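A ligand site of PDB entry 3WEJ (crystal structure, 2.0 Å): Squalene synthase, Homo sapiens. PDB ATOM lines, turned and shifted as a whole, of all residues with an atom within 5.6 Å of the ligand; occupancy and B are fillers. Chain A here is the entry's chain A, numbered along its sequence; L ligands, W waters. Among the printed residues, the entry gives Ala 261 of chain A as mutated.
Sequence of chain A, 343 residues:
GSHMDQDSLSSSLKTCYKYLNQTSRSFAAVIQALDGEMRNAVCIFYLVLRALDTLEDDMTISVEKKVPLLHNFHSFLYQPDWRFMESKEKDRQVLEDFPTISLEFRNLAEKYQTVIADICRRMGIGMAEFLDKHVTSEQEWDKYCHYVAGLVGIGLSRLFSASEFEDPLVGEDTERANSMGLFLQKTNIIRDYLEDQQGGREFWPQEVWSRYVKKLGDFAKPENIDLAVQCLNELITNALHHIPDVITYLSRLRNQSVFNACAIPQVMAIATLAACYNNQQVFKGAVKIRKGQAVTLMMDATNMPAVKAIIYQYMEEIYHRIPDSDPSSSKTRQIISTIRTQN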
ATOM      1  N   THR A  23     -17.557  -0.206 -31.532  1.00  0.00           N
ATOM      2  CA  THR A  23     -18.390  -1.362 -31.882  1.00  0.00           C
ATOM      3  C   THR A  23     -18.817  -2.273 -30.741  1.00  0.00           C
ATOM      4  O   THR A  23     -19.835  -2.942 -30.856  1.00  0.00           O
ATOM      5  CB  THR A  23     -17.768  -2.218 -33.009  1.00  0.00           C
ATOM      6  OG1 THR A  23     -16.544  -2.823 -32.563  1.00  0.00           O
ATOM      7  CG2 THR A  23     -17.508  -1.388 -34.282  1.00  0.00           C
ATOM      8  N   SER A  24     -18.052  -2.313 -29.653  1.00  0.00           N
ATOM      9  CA  SER A  24     -18.384  -3.174 -28.523  1.00  0.00           C
ATOM     10  C   SER A  24     -18.826  -2.459 -27.261  1.00  0.00           C
ATOM     11  O   SER A  24     -17.995  -1.926 -26.531  1.00  0.00           O
ATOM     12  CB  SER A  24     -17.224  -4.086 -28.119  1.00  0.00           C
ATOM     13  OG  SER A  24     -17.636  -4.881 -27.026  1.00  0.00           O
ATOM     14  N   ARG A  25     -20.126  -2.532 -26.963  1.00  0.00           N
ATOM     15  CA  ARG A  25     -20.670  -1.990 -25.720  1.00  0.00           C
ATOM     16  C   ARG A  25     -20.260  -2.828 -24.513  1.00  0.00           C
ATOM     17  O   ARG A  25     -19.855  -2.285 -23.484  1.00  0.00           O
ATOM     18  CB  ARG A  25     -22.193  -1.934 -25.808  1.00  0.00           C
ATOM     19  CG  ARG A  25     -22.848  -0.662 -25.257  1.00  0.00           C
ATOM     20  CD  ARG A  25     -22.619  -0.411 -23.765  1.00  0.00           C
ATOM     21  NE  ARG A  25     -21.362   0.279 -23.438  1.00  0.00           N
ATOM     22  CZ  ARG A  25     -20.795   1.267 -24.122  1.00  0.00           C
ATOM     23  NH1 ARG A  25     -21.349   1.748 -25.237  1.00  0.00           N
ATOM     24  NH2 ARG A  25     -19.657   1.799 -23.695  1.00  0.00           N
ATOM     25  N   SER A  26     -20.364  -4.141 -24.634  1.00  0.00           N
ATOM     26  CA  SER A  26     -20.188  -5.054 -23.512  1.00  0.00           C
ATOM     27  C   SER A  26     -18.726  -5.283 -23.128  1.00  0.00           C
ATOM     28  O   SER A  26     -18.436  -5.542 -21.964  1.00  0.00           O
ATOM     29  CB  SER A  26     -20.794  -6.420 -23.839  1.00  0.00           C
ATOM     30  OG  SER A  26     -22.205  -6.440 -23.678  1.00  0.00           O
ATOM     31  N   PHE A  27     -17.821  -5.209 -24.105  1.00  0.00           N
ATOM     32  CA  PHE A  27     -16.486  -5.774 -23.926  1.00  0.00           C
ATOM     33  C   PHE A  27     -15.307  -4.805 -23.933  1.00  0.00           C
ATOM     34  O   PHE A  27     -14.232  -5.165 -23.445  1.00  0.00           O
ATOM     35  CB  PHE A  27     -16.271  -6.919 -24.905  1.00  0.00           C
ATOM     36  CG  PHE A  27     -17.297  -8.003 -24.809  1.00  0.00           C
ATOM     37  CD1 PHE A  27     -17.569  -8.610 -23.589  1.00  0.00           C
ATOM     38  CD2 PHE A  27     -17.994  -8.429 -25.927  1.00  0.00           C
ATOM     39  CE1 PHE A  27     -18.520  -9.628 -23.492  1.00  0.00           C
ATOM     40  CE2 PHE A  27     -18.943  -9.446 -25.844  1.00  0.00           C
ATOM     41  CZ  PHE A  27     -19.202 -10.050 -24.622  1.00  0.00           C
ATOM     42  N   VAL A  30     -13.572  -4.119 -20.245  1.00  0.00           N
ATOM     43  CA  VAL A  30     -12.828  -5.250 -19.719  1.00  0.00           C
ATOM     44  C   VAL A  30     -11.636  -5.622 -20.591  1.00  0.00           C
ATOM     45  O   VAL A  30     -10.587  -5.998 -20.059  1.00  0.00           O
ATOM     46  CB  VAL A  30     -13.687  -6.491 -19.391  1.00  0.00           C
ATOM     47  CG1 VAL A  30     -14.671  -6.135 -18.271  1.00  0.00           C
ATOM     48  CG2 VAL A  30     -14.395  -7.038 -20.611  1.00  0.00           C
ATOM     49  N   ILE A  31     -11.772  -5.491 -21.911  1.00  0.00           N
ATOM     50  CA  ILE A  31     -10.650  -5.826 -22.799  1.00  0.00           C
ATOM     51  C   ILE A  31      -9.510  -4.839 -22.595  1.00  0.00           C
ATOM     52  O   ILE A  31      -8.344  -5.222 -22.489  1.00  0.00           O
ATOM     53  CB  ILE A  31     -11.071  -5.880 -24.289  1.00  0.00           C
ATOM     54  CG1 ILE A  31     -12.061  -7.040 -24.528  1.00  0.00           C
ATOM     55  CG2 ILE A  31      -9.845  -5.948 -25.195  1.00  0.00           C
ATOM     56  CD1 ILE A  31     -12.653  -7.079 -25.938  1.00  0.00           C
ATOM     57  N   LEU A  34      -7.231  -5.515 -19.604  1.00  0.00           N
ATOM     58  CA  LEU A  34      -6.360  -6.699 -19.592  1.00  0.00           C
ATOM     59  C   LEU A  34      -4.868  -6.374 -19.500  1.00  0.00           C
ATOM     60  O   LEU A  34      -4.370  -5.442 -20.141  1.00  0.00           O
ATOM     61  CB  LEU A  34      -6.615  -7.595 -20.796  1.00  0.00           C
ATOM     62  CG  LEU A  34      -7.929  -8.387 -20.800  1.00  0.00           C
ATOM     63  CD1 LEU A  34      -8.236  -8.777 -22.235  1.00  0.00           C
ATOM     64  CD2 LEU A  34      -7.843  -9.618 -19.898  1.00  0.00           C
ATOM     65  N   VAL A  42      -6.377  -9.757 -27.475  1.00  0.00           N
ATOM     66  CA  VAL A  42      -7.817  -9.822 -27.350  1.00  0.00           C
ATOM     67  C   VAL A  42      -8.522  -8.678 -28.077  1.00  0.00           C
ATOM     68  O   VAL A  42      -9.574  -8.882 -28.701  1.00  0.00           O
ATOM     69  CB  VAL A  42      -8.218  -9.931 -25.864  1.00  0.00           C
ATOM     70  CG1 VAL A  42      -9.736 -10.002 -25.744  1.00  0.00           C
ATOM     71  CG2 VAL A  42      -7.589 -11.199 -25.278  1.00  0.00           C
ATOM     72  N   PHE A  45      -8.457 -10.061 -31.590  1.00  0.00           N
ATOM     73  CA  PHE A  45      -9.332 -11.222 -31.689  1.00  0.00           C
ATOM     74  C   PHE A  45     -10.764 -10.738 -31.853  1.00  0.00           C
ATOM     75  O   PHE A  45     -11.484 -11.174 -32.746  1.00  0.00           O
ATOM     76  CB  PHE A  45      -9.231 -12.062 -30.424  1.00  0.00           C
ATOM     77  CG  PHE A  45     -10.021 -13.340 -30.459  1.00  0.00           C
ATOM     78  CD1 PHE A  45     -10.077 -14.117 -31.597  1.00  0.00           C
ATOM     79  CD2 PHE A  45     -10.647 -13.791 -29.316  1.00  0.00           C
ATOM     80  CE1 PHE A  45     -10.758 -15.343 -31.604  1.00  0.00           C
ATOM     81  CE2 PHE A  45     -11.335 -15.000 -29.295  1.00  0.00           C
ATOM     82  CZ  PHE A  45     -11.394 -15.786 -30.455  1.00  0.00           C
ATOM     83  N   TYR A  46     -11.151  -9.787 -31.013  1.00  0.00           N
ATOM     84  CA  TYR A  46     -12.463  -9.179 -31.079  1.00  0.00           C
ATOM     85  C   TYR A  46     -12.768  -8.581 -32.455  1.00  0.00           C
ATOM     86  O   TYR A  46     -13.821  -8.887 -33.042  1.00  0.00           O
ATOM     87  CB  TYR A  46     -12.657  -8.146 -29.966  1.00  0.00           C
ATOM     88  CG  TYR A  46     -13.927  -7.373 -30.167  1.00  0.00           C
ATOM     89  CD1 TYR A  46     -13.920  -6.219 -30.966  1.00  0.00           C
ATOM     90  CD2 TYR A  46     -15.138  -7.812 -29.632  1.00  0.00           C
ATOM     91  CE1 TYR A  46     -15.082  -5.526 -31.197  1.00  0.00           C
ATOM     92  CE2 TYR A  46     -16.311  -7.102 -29.856  1.00  0.00           C
ATOM     93  CZ  TYR A  46     -16.272  -5.971 -30.652  1.00  0.00           C
ATOM     94  OH  TYR A  46     -17.398  -5.220 -30.902  1.00  0.00           O
ATOM     95  N   LEU A  49     -13.199 -11.170 -35.371  1.00  0.00           N
ATOM     96  CA  LEU A  49     -14.500 -11.850 -35.274  1.00  0.00           C
ATOM     97  C   LEU A  49     -15.687 -10.917 -35.502  1.00  0.00           C
ATOM     98  O   LEU A  49     -16.712 -11.311 -36.025  1.00  0.00           O
ATOM     99  CB  LEU A  49     -14.642 -12.536 -33.917  1.00  0.00           C
ATOM    100  CG  LEU A  49     -13.683 -13.718 -33.697  1.00  0.00           C
ATOM    101  CD1 LEU A  49     -14.137 -14.543 -32.533  1.00  0.00           C
ATOM    102  CD2 LEU A  49     -13.575 -14.582 -34.927  1.00  0.00           C
ATOM    103  N   ARG A  50     -15.527  -9.661 -35.131  1.00  0.00           N
ATOM    104  CA  ARG A  50     -16.589  -8.693 -35.365  1.00  0.00           C
ATOM    105  C   ARG A  50     -16.755  -8.442 -36.862  1.00  0.00           C
ATOM    106  O   ARG A  50     -17.897  -8.381 -37.341  1.00  0.00           O
ATOM    107  CB  ARG A  50     -16.303  -7.403 -34.570  1.00  0.00           C
ATOM    108  CG  ARG A  50     -17.116  -6.177 -34.973  1.00  0.00           C
ATOM    109  CD  ARG A  50     -18.625  -6.310 -34.754  1.00  0.00           C
ATOM    110  NE  ARG A  50     -19.049  -6.837 -33.461  1.00  0.00           N
ATOM    111  CZ  ARG A  50     -20.082  -6.358 -32.751  1.00  0.00           C
ATOM    112  NH1 ARG A  50     -20.771  -5.300 -33.172  1.00  0.00           N
ATOM    113  NH2 ARG A  50     -20.400  -6.931 -31.602  1.00  0.00           N
ATOM    114  N   VAL A 148     -20.809 -19.814 -33.093  1.00  0.00           N
ATOM    115  CA  VAL A 148     -20.772 -18.352 -32.966  1.00  0.00           C
ATOM    116  C   VAL A 148     -20.302 -17.784 -31.617  1.00  0.00           C
ATOM    117  O   VAL A 148     -20.138 -16.572 -31.477  1.00  0.00           O
ATOM    118  CB  VAL A 148     -22.105 -17.709 -33.377  1.00  0.00           C
ATOM    119  CG1 VAL A 148     -22.450 -18.044 -34.829  1.00  0.00           C
ATOM    120  CG2 VAL A 148     -23.246 -18.184 -32.482  1.00  0.00           C
ATOM    121  N   ALA A 149     -20.086 -18.665 -30.637  1.00  0.00           N
ATOM    122  CA  ALA A 149     -19.871 -18.241 -29.251  1.00  0.00           C
ATOM    123  C   ALA A 149     -18.989 -19.187 -28.463  1.00  0.00           C
ATOM    124  O   ALA A 149     -18.073 -18.758 -27.769  1.00  0.00           O
ATOM    125  CB  ALA A 149     -21.218 -18.099 -28.539  1.00  0.00           C
ATOM    126  N   VAL A 152     -15.503 -18.649 -29.519  1.00  0.00           N
ATOM    127  CA  VAL A 152     -14.923 -17.447 -28.933  1.00  0.00           C
ATOM    128  C   VAL A 152     -14.351 -17.779 -27.542  1.00  0.00           C
ATOM    129  O   VAL A 152     -13.233 -17.361 -27.210  1.00  0.00           O
ATOM    130  CB  VAL A 152     -15.985 -16.356 -28.838  1.00  0.00           C
ATOM    131  CG1 VAL A 152     -15.361 -15.030 -28.396  1.00  0.00           C
ATOM    132  CG2 VAL A 152     -16.715 -16.231 -30.181  1.00  0.00           C
ATOM    133  N   GLY A 153     -15.089 -18.548 -26.750  1.00  0.00           N
ATOM    134  CA  GLY A 153     -14.637 -18.953 -25.426  1.00  0.00           C
ATOM    135  C   GLY A 153     -13.388 -19.804 -25.484  1.00  0.00           C
ATOM    136  O   GLY A 153     -12.431 -19.603 -24.732  1.00  0.00           O
ATOM    137  N   ILE A 154     -13.390 -20.749 -26.407  1.00  0.00           N
ATOM    138  CA  ILE A 154     -12.202 -21.587 -26.633  1.00  0.00           C
ATOM    139  C   ILE A 154     -11.008 -20.726 -27.081  1.00  0.00           C
ATOM    140  O   ILE A 154      -9.883 -20.923 -26.598  1.00  0.00           O
ATOM    141  CB  ILE A 154     -12.523 -22.716 -27.618  1.00  0.00           C
ATOM    142  CG1 ILE A 154     -13.494 -23.732 -26.978  1.00  0.00           C
ATOM    143  CG2 ILE A 154     -11.235 -23.417 -28.077  1.00  0.00           C
ATOM    144  CD1 ILE A 154     -14.235 -24.607 -28.015  1.00  0.00           C
ATOM    145  N   LEU A 156     -10.563 -17.305 -26.567  1.00  0.00           N
ATOM    146  CA  LEU A 156     -10.099 -16.529 -25.422  1.00  0.00           C
ATOM    147  C   LEU A 156      -9.279 -17.391 -24.452  1.00  0.00           C
ATOM    148  O   LEU A 156      -8.209 -16.996 -24.022  1.00  0.00           O
ATOM    149  CB  LEU A 156     -11.255 -15.851 -24.685  1.00  0.00           C
ATOM    150  CG  LEU A 156     -11.936 -14.702 -25.429  1.00  0.00           C
ATOM    151  CD1 LEU A 156     -13.198 -14.228 -24.691  1.00  0.00           C
ATOM    152  CD2 LEU A 156     -10.959 -13.553 -25.658  1.00  0.00           C
ATOM    153  N   SER A 157      -9.758 -18.586 -24.175  1.00  0.00           N
ATOM    154  CA  SER A 157      -9.080 -19.475 -23.237  1.00  0.00           C
ATOM    155  C   SER A 157      -7.657 -19.802 -23.675  1.00  0.00           C
ATOM    156  O   SER A 157      -6.752 -19.838 -22.859  1.00  0.00           O
ATOM    157  CB  SER A 157      -9.870 -20.779 -23.073  1.00  0.00           C
ATOM    158  OG  SER A 157     -11.154 -20.477 -22.571  1.00  0.00           O
ATOM    159  N   PHE A 160      -5.415 -16.777 -23.228  1.00  0.00           N
ATOM    160  CA  PHE A 160      -5.044 -16.578 -21.816  1.00  0.00           C
ATOM    161  C   PHE A 160      -3.891 -17.511 -21.428  1.00  0.00           C
ATOM    162  O   PHE A 160      -2.922 -17.090 -20.783  1.00  0.00           O
ATOM    163  CB  PHE A 160      -6.206 -16.855 -20.855  1.00  0.00           C
ATOM    164  CG  PHE A 160      -7.382 -15.952 -21.026  1.00  0.00           C
ATOM    165  CD1 PHE A 160      -7.221 -14.616 -21.352  1.00  0.00           C
ATOM    166  CD2 PHE A 160      -8.670 -16.429 -20.814  1.00  0.00           C
ATOM    167  CE1 PHE A 160      -8.312 -13.769 -21.491  1.00  0.00           C
ATOM    168  CE2 PHE A 160      -9.764 -15.603 -20.947  1.00  0.00           C
ATOM    169  CZ  PHE A 160      -9.593 -14.264 -21.294  1.00  0.00           C
ATOM    170  N   ALA A 177     -14.711 -24.098 -21.606  1.00  0.00           N
ATOM    171  CA  ALA A 177     -14.682 -22.848 -22.346  1.00  0.00           C
ATOM    172  C   ALA A 177     -15.872 -22.712 -23.317  1.00  0.00           C
ATOM    173  O   ALA A 177     -16.415 -21.623 -23.476  1.00  0.00           O
ATOM    174  CB  ALA A 177     -13.364 -22.698 -23.096  1.00  0.00           C
ATOM    175  N   MET A 180     -19.042 -21.640 -21.414  1.00  0.00           N
ATOM    176  CA  MET A 180     -18.991 -20.209 -21.121  1.00  0.00           C
ATOM    177  C   MET A 180     -19.628 -19.398 -22.251  1.00  0.00           C
ATOM    178  O   MET A 180     -20.473 -18.543 -21.999  1.00  0.00           O
ATOM    179  CB  MET A 180     -17.547 -19.765 -20.887  1.00  0.00           C
ATOM    180  CG  MET A 180     -16.933 -20.219 -19.561  1.00  0.00           C
ATOM    181  SD  MET A 180     -17.352 -19.229 -18.100  1.00  0.00           S
ATOM    182  CE  MET A 180     -16.670 -17.614 -18.506  1.00  0.00           C
ATOM    183  N   GLY A 181     -19.229 -19.684 -23.495  1.00  0.00           N
ATOM    184  CA  GLY A 181     -19.794 -19.071 -24.690  1.00  0.00           C
ATOM    185  C   GLY A 181     -21.250 -19.437 -24.900  1.00  0.00           C
ATOM    186  O   GLY A 181     -22.067 -18.571 -25.209  1.00  0.00           O
ATOM    187  N   LEU A 184     -23.546 -17.386 -22.557  1.00  0.00           N
ATOM    188  CA  LEU A 184     -23.740 -15.995 -23.009  1.00  0.00           C
ATOM    189  C   LEU A 184     -24.655 -15.930 -24.227  1.00  0.00           C
ATOM    190  O   LEU A 184     -25.525 -15.082 -24.287  1.00  0.00           O
ATOM    191  CB  LEU A 184     -22.424 -15.296 -23.340  1.00  0.00           C
ATOM    192  CG  LEU A 184     -21.451 -15.030 -22.201  1.00  0.00           C
ATOM    193  CD1 LEU A 184     -20.489 -13.939 -22.658  1.00  0.00           C
ATOM    194  CD2 LEU A 184     -22.178 -14.617 -20.937  1.00  0.00           C
ATOM    195  N   GLN A 185     -24.455 -16.855 -25.160  1.00  0.00           N
ATOM    196  CA  GLN A 185     -25.153 -16.797 -26.443  1.00  0.00           C
ATOM    197  C   GLN A 185     -26.640 -17.137 -26.327  1.00  0.00           C
ATOM    198  O   GLN A 185     -27.478 -16.432 -26.886  1.00  0.00           O
ATOM    199  CB  GLN A 185     -24.475 -17.653 -27.512  1.00  0.00           C
ATOM    200  CG  GLN A 185     -25.071 -17.500 -28.903  1.00  0.00           C
ATOM    201  CD  GLN A 185     -24.647 -16.215 -29.556  1.00  0.00           C
ATOM    202  OE1 GLN A 185     -25.350 -15.214 -29.531  1.00  0.00           O
ATOM    203  NE2 GLN A 185     -23.446 -16.226 -30.119  1.00  0.00           N
ATOM    204  N   ASN A 188     -28.524 -14.198 -24.756  1.00  0.00           N
ATOM    205  CA  ASN A 188     -28.785 -13.172 -25.771  1.00  0.00           C
ATOM    206  C   ASN A 188     -29.935 -13.529 -26.713  1.00  0.00           C
ATOM    207  O   ASN A 188     -30.803 -12.715 -27.005  1.00  0.00           O
ATOM    208  CB  ASN A 188     -27.527 -12.919 -26.624  1.00  0.00           C
ATOM    209  CG  ASN A 188     -26.446 -12.122 -25.904  1.00  0.00           C
ATOM    210  OD1 ASN A 188     -26.696 -11.474 -24.880  1.00  0.00           O
ATOM    211  ND2 ASN A 188     -25.221 -12.180 -26.429  1.00  0.00           N
ATOM    212  N   TYR A 249     -15.103 -23.013 -14.684  1.00  0.00           N
ATOM    213  CA  TYR A 249     -14.176 -22.246 -15.510  1.00  0.00           C
ATOM    214  C   TYR A 249     -13.630 -21.067 -14.702  1.00  0.00           C
ATOM    215  O   TYR A 249     -12.405 -20.929 -14.549  1.00  0.00           O
ATOM    216  CB  TYR A 249     -14.860 -21.777 -16.790  1.00  0.00           C
ATOM    217  CG  TYR A 249     -13.947 -21.029 -17.727  1.00  0.00           C
ATOM    218  CD1 TYR A 249     -13.792 -19.645 -17.600  1.00  0.00           C
ATOM    219  CD2 TYR A 249     -13.239 -21.688 -18.728  1.00  0.00           C
ATOM    220  CE1 TYR A 249     -12.944 -18.955 -18.436  1.00  0.00           C
ATOM    221  CE2 TYR A 249     -12.389 -20.996 -19.578  1.00  0.00           C
ATOM    222  CZ  TYR A 249     -12.243 -19.635 -19.418  1.00  0.00           C
ATOM    223  OH  TYR A 249     -11.410 -18.917 -20.233  1.00  0.00           O
ATOM    224  N   ALA A 261     -12.717  -9.999 -16.751  1.00  0.00           N
ATOM    225  CA  ALA A 261     -13.147 -10.027 -18.141  1.00  0.00           C
ATOM    226  C   ALA A 261     -14.093 -11.197 -18.410  1.00  0.00           C
ATOM    227  O   ALA A 261     -15.041 -11.091 -19.179  1.00  0.00           O
ATOM    228  CB  ALA A 261     -11.941 -10.089 -19.057  1.00  0.00           C
ATOM    229  N   CYS A 262     -13.806 -12.330 -17.771  1.00  0.00           N
ATOM    230  CA  CYS A 262     -14.621 -13.509 -17.898  1.00  0.00           C
ATOM    231  C   CYS A 262     -15.881 -13.478 -17.013  1.00  0.00           C
ATOM    232  O   CYS A 262     -16.943 -13.943 -17.453  1.00  0.00           O
ATOM    233  CB  CYS A 262     -13.770 -14.726 -17.560  1.00  0.00           C
ATOM    234  SG  CYS A 262     -12.488 -14.998 -18.814  1.00  0.00           S
ATOM    235  N   PRO A 265     -19.331 -10.552 -17.851  1.00  0.00           N
ATOM    236  CA  PRO A 265     -20.372 -10.948 -18.793  1.00  0.00           C
ATOM    237  C   PRO A 265     -21.171 -12.160 -18.338  1.00  0.00           C
ATOM    238  O   PRO A 265     -22.321 -12.287 -18.730  1.00  0.00           O
ATOM    239  CB  PRO A 265     -19.578 -11.287 -20.063  1.00  0.00           C
ATOM    240  CG  PRO A 265     -18.324 -10.479 -19.946  1.00  0.00           C
ATOM    241  CD  PRO A 265     -18.006 -10.577 -18.488  1.00  0.00           C
ATOM    242  N   GLN A 266     -20.591 -13.045 -17.516  1.00  0.00           N
ATOM    243  CA  GLN A 266     -21.364 -14.201 -17.061  1.00  0.00           C
ATOM    244  C   GLN A 266     -22.416 -13.774 -16.049  1.00  0.00           C
ATOM    245  O   GLN A 266     -23.579 -14.156 -16.156  1.00  0.00           O
ATOM    246  CB  GLN A 266     -20.461 -15.282 -16.456  1.00  0.00           C
ATOM    247  CG  GLN A 266     -19.505 -15.850 -17.471  1.00  0.00           C
ATOM    248  CD  GLN A 266     -20.198 -16.496 -18.666  1.00  0.00           C
ATOM    249  OE1 GLN A 266     -19.745 -16.366 -19.798  1.00  0.00           O
ATOM    250  NE2 GLN A 266     -21.298 -17.192 -18.401  1.00  0.00           N
HETATM  251  C1  LIG L   1     -12.745 -10.596 -23.654  1.00  0.00           C
HETATM  252  C2  LIG L   1     -14.987 -11.036 -22.344  1.00  0.00           C
HETATM  253  C3  LIG L   1     -14.443 -18.439 -21.800  1.00  0.00           C
HETATM  254  C4  LIG L   1     -14.771 -15.826 -21.657  1.00  0.00           C
HETATM  255  C5  LIG L   1     -13.516 -11.733 -28.842  1.00  0.00           C
HETATM  256  C6  LIG L   1     -17.533 -13.578 -25.200  1.00  0.00           C
HETATM  257  C7  LIG L   1     -18.939  -9.968 -31.095  1.00  0.00           C
HETATM  258  C8  LIG L   1     -22.595 -13.482 -28.389  1.00  0.00           C
HETATM  259  O1  LIG L   1     -21.520  -5.243 -27.135  1.00  0.00           O
HETATM  260  O2  LIG L   1     -23.414  -8.249 -25.704  1.00  0.00           O
HETATM  261  O3  LIG L   1     -19.559  -6.421 -28.383  1.00  0.00           O
HETATM  262  O4  LIG L   1     -21.943  -6.482 -29.362  1.00  0.00           O
HETATM  263  O5  LIG L   1     -23.792  -8.022 -28.240  1.00  0.00           O
HETATM  264  C9  LIG L   1     -15.015 -10.771 -24.836  1.00  0.00           C
HETATM  265  C10 LIG L   1     -16.308 -17.308 -23.071  1.00  0.00           C
HETATM  266  C11 LIG L   1     -16.021 -11.400 -29.437  1.00  0.00           C
HETATM  267  C12 LIG L   1     -19.095 -15.279 -26.265  1.00  0.00           C
HETATM  268  C13 LIG L   1     -19.381 -12.431 -30.405  1.00  0.00           C
HETATM  269  C14 LIG L   1     -14.573 -10.588 -26.139  1.00  0.00           C
HETATM  270  C15 LIG L   1     -17.151 -16.330 -23.571  1.00  0.00           C
HETATM  271  C16 LIG L   1     -15.982 -11.396 -30.829  1.00  0.00           C
HETATM  272  C17 LIG L   1     -20.059 -14.358 -26.674  1.00  0.00           C
HETATM  273  C18 LIG L   1     -15.448 -11.452 -27.046  1.00  0.00           C
HETATM  274  C19 LIG L   1     -17.025 -16.173 -25.091  1.00  0.00           C
HETATM  275  C20 LIG L   1     -17.230 -11.973 -31.506  1.00  0.00           C
HETATM  276  C21 LIG L   1     -22.078 -10.559 -28.545  1.00  0.00           C
HETATM  277  C22 LIG L   1     -20.078 -14.078 -28.166  1.00  0.00           C
HETATM  278  O6  LIG L   1     -22.570 -10.120 -27.278  1.00  0.00           O
HETATM  279  O7  LIG L   1     -21.353  -7.849 -27.239  1.00  0.00           O
HETATM  280  C23 LIG L   1     -14.266 -10.806 -23.665  1.00  0.00           C
HETATM  281  C24 LIG L   1     -15.200 -17.181 -22.220  1.00  0.00           C
HETATM  282  C25 LIG L   1     -14.999 -11.507 -28.499  1.00  0.00           C
HETATM  283  C26 LIG L   1     -17.922 -15.013 -25.561  1.00  0.00           C
HETATM  284  C27 LIG L   1     -18.561 -11.457 -30.971  1.00  0.00           C
HETATM  285  C28 LIG L   1     -20.782 -12.225 -29.834  1.00  0.00           C
HETATM  286  C29 LIG L   1     -20.880 -11.516 -28.482  1.00  0.00           C
HETATM  287  C30 LIG L   1     -21.145 -13.035 -28.577  1.00  0.00           C
HETATM  288  P1  LIG L   1     -20.999  -6.482 -28.049  1.00  0.00           P
HETATM  289  P2  LIG L   1     -22.821  -8.514 -27.038  1.00  0.00           P
HETATM  290  O   HOH W   1     -17.607 -14.555 -20.098  1.00  0.00           O
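An oxygen (O4) of the ligand is in salt-bridge range of the guanidinium group (NH2) of Arg 50, at 2.8 Å. The side-chain hydroxyl (OG) of Ser 24 is in hydrogen-bond range of an oxygen (O3) of the ligand, 2.8 Å away. The backbone NH (N) of Ser 26 lies within hydrogen-bond range of an oxygen (O1) of the ligand (3.0 Å). O2 of the ligand lies within hydrogen-bond range of OG of Ser 26. N of Arg 25 lies within hydrogen-bond range of O1 of the ligand. An oxygen (O6) of the ligand is in hydrogen-bond range of the side-chain amide nitrogen (ND2) of Asn 188, at 3.5 Å.
OH of Tyr 46 sits at hydrogen-bond distance from NE of Arg 50 (3.4 Å). The guanidinium group (NH1) of Arg 50 is in hydrogen-bond range of the backbone carbonyl oxygen (O) of Thr 23 (3.4 Å). OG of Ser 24 is in hydrogen-bond range of N of Phe 27 (2.9 Å). The backbone NH (N) of Ser 24 sits close to the side-chain hydroxyl (OH) of Tyr 46 (3.2 Å). The side-chain hydroxyl (OG) of Ser 157 sits at hydrogen-bond distance from the backbone carbonyl oxygen (O) of Gly 153. OH of Tyr 249 is in hydrogen-bond range of OG of Ser 157. The side-chain amide oxygen (OE1) of Gln 266 sits close to the backbone carbonyl oxygen (O) of Met 180, at 3.2 Å. The side-chain hydroxyl (OH) of Tyr 46 sits at hydrogen-bond distance from the side-chain hydroxyl (OG1) of Thr 23, 3.0 Å away.
CE2 of Phe 27 touches O7 of the ligand, 3.2 Å away. CG1 of Ile 31 touches C1 of the ligand (3.7 Å). Val 42 touches the ligand (CG1 to C1, 3.7 Å). Phe 45 touches the ligand. Tyr 46 touches the ligand. Leu 49 touches the ligand (CB to C16, 3.6 Å). Ala 149 touches the ligand (O to C19, 3.9 Å). Val 152 touches the ligand (CG1 to C25, 3.5 Å). Gly 153 touches the ligand (CA to C10, 3.3 Å). Leu 156 touches the ligand (CD1 to C23, 3.7 Å). OG of Ser 157 touches C3 of the ligand (3.9 Å). Met 180 touches the ligand. N of Gly 181 touches C10 of the ligand, 3.8 Å away. Leu 184 touches the ligand. Gln 185 touches the ligand (NE2 to C8, 3.4 Å). OH of Tyr 249 touches C3 of the ligand, 3.4 Å away. O of Ala 261 touches C2 of the ligand, at 3.2 Å. Cys 262 touches the ligand. Hydrophobic or aromatic side chains within 4 Å of the ligand: Phe 27, Ile 31, Val 42, Phe 45, Tyr 46, Leu 49, Val 152, Leu 156, Met 180, Leu 184 and Tyr 249. Within 4 Å of the ligand: Ser 24, Arg 25, Ser 26, Phe 27, Ile 31, Val 42, Phe 45, Tyr 46, Leu 49, Arg 50, Ala 149, Val 152, Gly 153, Leu 156, Ser 157, Met 180, Gly 181, Leu 184, Gln 185, Asn 188, Tyr 249, Ala 261 and Cys 262. The nearest printed residue that does not touch the ligand is Ala 177 (4.1 Å).
Water W1 bridges O of Cys 262 (2.8 Å) and OE1 of Gln 266 (2.8 Å).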
